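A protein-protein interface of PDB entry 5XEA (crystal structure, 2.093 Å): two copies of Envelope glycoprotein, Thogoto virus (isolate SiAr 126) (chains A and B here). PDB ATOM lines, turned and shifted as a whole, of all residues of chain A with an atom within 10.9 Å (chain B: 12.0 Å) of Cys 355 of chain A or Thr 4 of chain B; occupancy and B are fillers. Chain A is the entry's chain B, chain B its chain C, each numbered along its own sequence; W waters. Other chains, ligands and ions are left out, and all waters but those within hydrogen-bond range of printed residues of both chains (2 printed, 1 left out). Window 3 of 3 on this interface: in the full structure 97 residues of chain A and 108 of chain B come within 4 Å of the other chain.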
ATOM      1  N   ALA A 338      20.619  -3.615   3.119  1.00  0.00           N
ATOM      2  CA  ALA A 338      20.310  -4.987   2.753  1.00  0.00           C
ATOM      3  C   ALA A 338      19.234  -5.494   3.695  1.00  0.00           C
ATOM      4  O   ALA A 338      19.252  -5.132   4.880  1.00  0.00           O
ATOM      5  CB  ALA A 338      21.553  -5.879   2.824  1.00  0.00           C
ATOM      6  N   PRO A 339      18.272  -6.321   3.215  1.00  0.00           N
ATOM      7  CA  PRO A 339      17.173  -6.780   4.087  1.00  0.00           C
ATOM      8  C   PRO A 339      17.595  -7.953   4.966  1.00  0.00           C
ATOM      9  O   PRO A 339      17.151  -9.094   4.805  1.00  0.00           O
ATOM     10  CB  PRO A 339      16.091  -7.156   3.068  1.00  0.00           C
ATOM     11  CG  PRO A 339      16.868  -7.660   1.889  1.00  0.00           C
ATOM     12  CD  PRO A 339      18.143  -6.841   1.840  1.00  0.00           C
ATOM     13  N   VAL A 340      18.485  -7.682   5.927  1.00  0.00           N
ATOM     14  CA  VAL A 340      19.012  -8.718   6.806  1.00  0.00           C
ATOM     15  C   VAL A 340      18.880  -8.288   8.264  1.00  0.00           C
ATOM     16  O   VAL A 340      18.928  -7.098   8.590  1.00  0.00           O
ATOM     17  CB  VAL A 340      20.492  -9.075   6.488  1.00  0.00           C
ATOM     18  CG1 VAL A 340      20.609  -9.757   5.136  1.00  0.00           C
ATOM     19  CG2 VAL A 340      21.396  -7.848   6.563  1.00  0.00           C
ATOM     20  N   SER A 341      18.705  -9.280   9.143  1.00  0.00           N
ATOM     21  CA  SER A 341      18.890  -9.125  10.580  1.00  0.00           C
ATOM     22  C   SER A 341      20.156  -9.864  11.002  1.00  0.00           C
ATOM     23  O   SER A 341      20.522 -10.879  10.402  1.00  0.00           O
ATOM     24  CB  SER A 341      17.695  -9.673  11.355  1.00  0.00           C
ATOM     25  OG  SER A 341      17.716 -11.086  11.314  1.00  0.00           O
ATOM     26  N   SER A 342      20.828  -9.354  12.031  1.00  0.00           N
ATOM     27  CA  SER A 342      22.098  -9.907  12.480  1.00  0.00           C
ATOM     28  C   SER A 342      21.933 -10.724  13.764  1.00  0.00           C
ATOM     29  O   SER A 342      20.956 -10.593  14.492  1.00  0.00           O
ATOM     30  CB  SER A 342      23.117  -8.802  12.724  1.00  0.00           C
ATOM     31  OG  SER A 342      22.656  -7.914  13.724  1.00  0.00           O
ATOM     32  N   LEU A 352      24.308 -13.214   9.489  1.00  0.00           N
ATOM     33  CA  LEU A 352      23.243 -12.458   8.848  1.00  0.00           C
ATOM     34  C   LEU A 352      22.139 -13.415   8.429  1.00  0.00           C
ATOM     35  O   LEU A 352      22.394 -14.413   7.742  1.00  0.00           O
ATOM     36  CB  LEU A 352      23.777 -11.666   7.646  1.00  0.00           C
ATOM     37  CG  LEU A 352      24.696 -10.490   7.991  1.00  0.00           C
ATOM     38  CD1 LEU A 352      25.242  -9.839   6.735  1.00  0.00           C
ATOM     39  CD2 LEU A 352      23.962  -9.451   8.856  1.00  0.00           C
ATOM     40  N   HIS A 353      20.917 -13.113   8.847  1.00  0.00           N
ATOM     41  CA  HIS A 353      19.751 -13.892   8.459  1.00  0.00           C
ATOM     42  C   HIS A 353      18.999 -13.160   7.358  1.00  0.00           C
ATOM     43  O   HIS A 353      18.822 -11.942   7.434  1.00  0.00           O
ATOM     44  CB  HIS A 353      18.820 -14.133   9.653  1.00  0.00           C
ATOM     45  CG  HIS A 353      19.456 -14.901  10.769  1.00  0.00           C
ATOM     46  ND1 HIS A 353      19.803 -16.231  10.660  1.00  0.00           N
ATOM     47  CD2 HIS A 353      19.801 -14.523  12.021  1.00  0.00           C
ATOM     48  CE1 HIS A 353      20.356 -16.634  11.791  1.00  0.00           C
ATOM     49  NE2 HIS A 353      20.364 -15.617  12.633  1.00  0.00           N
ATOM     50  N   GLN A 354      18.537 -13.903   6.353  1.00  0.00           N
ATOM     51  CA  GLN A 354      17.885 -13.320   5.194  1.00  0.00           C
ATOM     52  C   GLN A 354      16.594 -14.069   4.877  1.00  0.00           C
ATOM     53  O   GLN A 354      16.359 -15.179   5.347  1.00  0.00           O
ATOM     54  CB  GLN A 354      18.817 -13.343   3.981  1.00  0.00           C
ATOM     55  CG  GLN A 354      18.522 -12.241   2.973  1.00  0.00           C
ATOM     56  CD  GLN A 354      19.309 -12.384   1.692  1.00  0.00           C
ATOM     57  OE1 GLN A 354      20.417 -12.916   1.693  1.00  0.00           O
ATOM     58  NE2 GLN A 354      18.730 -11.925   0.583  1.00  0.00           N
ATOM     59  N   CYS A 355      15.777 -13.440   4.032  1.00  0.00           N
ATOM     60  CA  CYS A 355      14.485 -13.948   3.528  1.00  0.00           C
ATOM     61  C   CYS A 355      13.630 -14.508   4.675  1.00  0.00           C
ATOM     62  O   CYS A 355      12.681 -13.851   5.116  1.00  0.00           O
ATOM     63  CB  CYS A 355      14.721 -14.998   2.432  1.00  0.00           C
ATOM     64  SG  CYS A 355      13.878 -16.598   2.605  1.00  0.00           S
ATOM     65  N   ASP B   1       8.091 -19.598  -0.084  1.00  0.00           N
ATOM     66  CA  ASP B   1       8.216 -20.420   1.114  1.00  0.00           C
ATOM     67  C   ASP B   1       9.123 -19.776   2.156  1.00  0.00           C
ATOM     68  O   ASP B   1       9.535 -20.437   3.112  1.00  0.00           O
ATOM     69  CB  ASP B   1       8.752 -21.811   0.758  1.00  0.00           C
ATOM     70  CG  ASP B   1       7.646 -22.812   0.489  1.00  0.00           C
ATOM     71  OD1 ASP B   1       6.534 -22.387   0.112  1.00  0.00           O
ATOM     72  OD2 ASP B   1       7.890 -24.026   0.657  1.00  0.00           O
ATOM     73  N   CYS B   2       9.416 -18.482   1.991  1.00  0.00           N
ATOM     74  CA  CYS B   2      10.354 -17.798   2.880  1.00  0.00           C
ATOM     75  C   CYS B   2       9.769 -17.576   4.273  1.00  0.00           C
ATOM     76  O   CYS B   2      10.028 -16.547   4.909  1.00  0.00           O
ATOM     77  CB  CYS B   2      10.813 -16.463   2.275  1.00  0.00           C
ATOM     78  SG  CYS B   2      12.336 -16.571   1.270  1.00  0.00           S
ATOM     79  N   ASN B   3       8.965 -18.532   4.747  1.00  0.00           N
ATOM     80  CA  ASN B   3       8.734 -18.667   6.179  1.00  0.00           C
ATOM     81  C   ASN B   3      10.029 -19.021   6.895  1.00  0.00           C
ATOM     82  O   ASN B   3      10.225 -18.648   8.058  1.00  0.00           O
ATOM     83  CB  ASN B   3       7.671 -19.739   6.428  1.00  0.00           C
ATOM     84  CG  ASN B   3       7.118 -19.710   7.838  1.00  0.00           C
ATOM     85  OD1 ASN B   3       7.620 -18.998   8.707  1.00  0.00           O
ATOM     86  ND2 ASN B   3       6.075 -20.500   8.074  1.00  0.00           N
ATOM     87  N   THR B   4      10.928 -19.721   6.203  1.00  0.00           N
ATOM     88  CA  THR B   4      12.221 -20.121   6.737  1.00  0.00           C
ATOM     89  C   THR B   4      13.277 -19.062   6.436  1.00  0.00           C
ATOM     90  O   THR B   4      13.296 -18.473   5.352  1.00  0.00           O
ATOM     91  CB  THR B   4      12.650 -21.463   6.137  1.00  0.00           C
ATOM     92  OG1 THR B   4      12.989 -21.282   4.754  1.00  0.00           O
ATOM     93  CG2 THR B   4      11.519 -22.477   6.234  1.00  0.00           C
ATOM     94  N   LYS B   5      14.164 -18.830   7.401  1.00  0.00           N
ATOM     95  CA  LYS B   5      15.254 -17.880   7.248  1.00  0.00           C
ATOM     96  C   LYS B   5      16.562 -18.620   7.020  1.00  0.00           C
ATOM     97  O   LYS B   5      16.802 -19.678   7.607  1.00  0.00           O
ATOM     98  CB  LYS B   5      15.384 -16.971   8.472  1.00  0.00           C
ATOM     99  CG  LYS B   5      14.435 -15.788   8.474  1.00  0.00           C
ATOM    100  CD  LYS B   5      14.908 -14.714   9.441  1.00  0.00           C
ATOM    101  CE  LYS B   5      13.988 -14.591  10.643  1.00  0.00           C
ATOM    102  NZ  LYS B   5      12.662 -13.994  10.308  1.00  0.00           N
ATOM    103  N   THR B   6      17.404 -18.059   6.166  1.00  0.00           N
ATOM    104  CA  THR B   6      18.727 -18.597   5.918  1.00  0.00           C
ATOM    105  C   THR B   6      19.761 -17.787   6.694  1.00  0.00           C
ATOM    106  O   THR B   6      19.525 -16.641   7.075  1.00  0.00           O
ATOM    107  CB  THR B   6      19.037 -18.587   4.418  1.00  0.00           C
ATOM    108  OG1 THR B   6      20.313 -19.197   4.186  1.00  0.00           O
ATOM    109  CG2 THR B   6      19.053 -17.154   3.882  1.00  0.00           C
ATOM    110  N   ALA B   7      20.909 -18.406   6.949  1.00  0.00           N
ATOM    111  CA  ALA B   7      21.968 -17.789   7.737  1.00  0.00           C
ATOM    112  C   ALA B   7      23.291 -17.914   7.002  1.00  0.00           C
ATOM    113  O   ALA B   7      23.634 -18.998   6.521  1.00  0.00           O
ATOM    114  CB  ALA B   7      22.075 -18.436   9.123  1.00  0.00           C
ATOM    115  N   THR B   8      24.025 -16.801   6.907  1.00  0.00           N
ATOM    116  CA  THR B   8      25.388 -16.783   6.384  1.00  0.00           C
ATOM    117  C   THR B   8      26.305 -16.101   7.385  1.00  0.00           C
ATOM    118  O   THR B   8      25.858 -15.380   8.281  1.00  0.00           O
ATOM    119  CB  THR B   8      25.505 -16.035   5.043  1.00  0.00           C
ATOM    120  OG1 THR B   8      24.961 -14.716   5.196  1.00  0.00           O
ATOM    121  CG2 THR B   8      24.783 -16.783   3.928  1.00  0.00           C
ATOM    122  N   TYR B  11      30.270 -12.662   9.810  1.00  0.00           N
ATOM    123  CA  TYR B  11      30.861 -11.459   9.247  1.00  0.00           C
ATOM    124  C   TYR B  11      31.483 -10.626  10.358  1.00  0.00           C
ATOM    125  O   TYR B  11      31.288 -10.876  11.549  1.00  0.00           O
ATOM    126  CB  TYR B  11      29.822 -10.620   8.500  1.00  0.00           C
ATOM    127  CG  TYR B  11      29.090 -11.324   7.383  1.00  0.00           C
ATOM    128  CD1 TYR B  11      29.537 -11.238   6.071  1.00  0.00           C
ATOM    129  CD2 TYR B  11      27.920 -12.048   7.635  1.00  0.00           C
ATOM    130  CE1 TYR B  11      28.864 -11.874   5.040  1.00  0.00           C
ATOM    131  CE2 TYR B  11      27.241 -12.681   6.610  1.00  0.00           C
ATOM    132  CZ  TYR B  11      27.720 -12.593   5.313  1.00  0.00           C
ATOM    133  OH  TYR B  11      27.042 -13.223   4.287  1.00  0.00           O
HETATM  134  O   HOH W   1      22.405 -14.346   4.792  1.00  0.00           O
HETATM  135  O   HOH W   2      18.584 -18.824   9.369  1.00  0.00           O
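N of Leu 352 of chain A is in hydrogen-bond range of O of Thr 8 of chain B.
The backbone carbonyl oxygen (O) of Thr 6 of chain B sits at hydrogen-bond distance from the backbone NH (N) of Gln 354 of chain A (3.0 Å).
The side-chain sulfur (SG) of Cys 355 of chain A forms a disulfide with the side-chain sulfur (SG) of Cys 2 of chain B, 2.0 Å away.
The backbone carbonyl oxygen of Thr 4 of chain B lies close to the side-chain sulfur of Cys 355 of chain A, 3.4 Å away.
N of His 353 of chain A lies within hydrogen-bond range of O of Ser 341 of chain A (2.8 Å).
The side-chain hydroxyl of Thr 8 of chain B is in hydrogen-bond range of the side-chain hydroxyl of Tyr 11 of chain B.
Among the printed residues, merely in contact across the chains: His 353 of chain A with Thr 6 of chain B (3.1 Å), Leu 352 of chain A with Ala 7 of chain B (3.4 Å), Leu 352 of chain A with Tyr 11 of chain B (3.5 Å), Gln 354 of chain A with Lys 5 of chain B (3.5 Å), His 353 of chain A with Ala 7 of chain B (3.5 Å), Leu 352 of chain A with Thr 6 of chain B (3.7 Å) and His 353 of chain A with Lys 5 of chain B (3.96 Å).
No residue of chain B comes within 4 Å of Pro 339 of chain A.
Of the printed residues of chain B, Cys 355 of chain A touches Cys 2 and Thr 4.
No residue of chain A comes within 4 Å of Asn 3 of chain B.
Of chain A, only Cys 355 comes within 4 Å of Thr 4 of chain B.
Of the printed residues of chain A, Lys 5 of chain B touches His 353 and Gln 354.
Printed residues of chain A within 4 Å of Thr 6 of chain B: Leu 352 (3.7 Å), His 353 (3.1 Å) and Gln 354 (3.0 Å).
Of the printed residues of chain A, Thr 8 of chain B touches Leu 352.
The nearest residue of chain B that does not touch Cys 355 of chain A is Lys 5 of chain B (4.1 Å).
Of the 9 printed residues of chain A, 4 touch a printed residue of chain B.
Along chain A the printed residues that touch a printed residue of chain B span positions 352 to 355.
No position is printed for both chains.
Water W1 lies within hydrogen-bond range of OG1 of Thr 8 of chain B and O of Leu 352 of chain A.
Water W2 lies within hydrogen-bond range of the backbone carbonyl oxygen of Lys 5 of chain B (2.6 Å), a ring nitrogen (ND1) of His 353 of chain A (3.1 Å), the backbone carbonyl oxygen of Thr 6 of chain B (3.3 Å) and the backbone NH of Ala 7 of chain B (3.4 Å).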
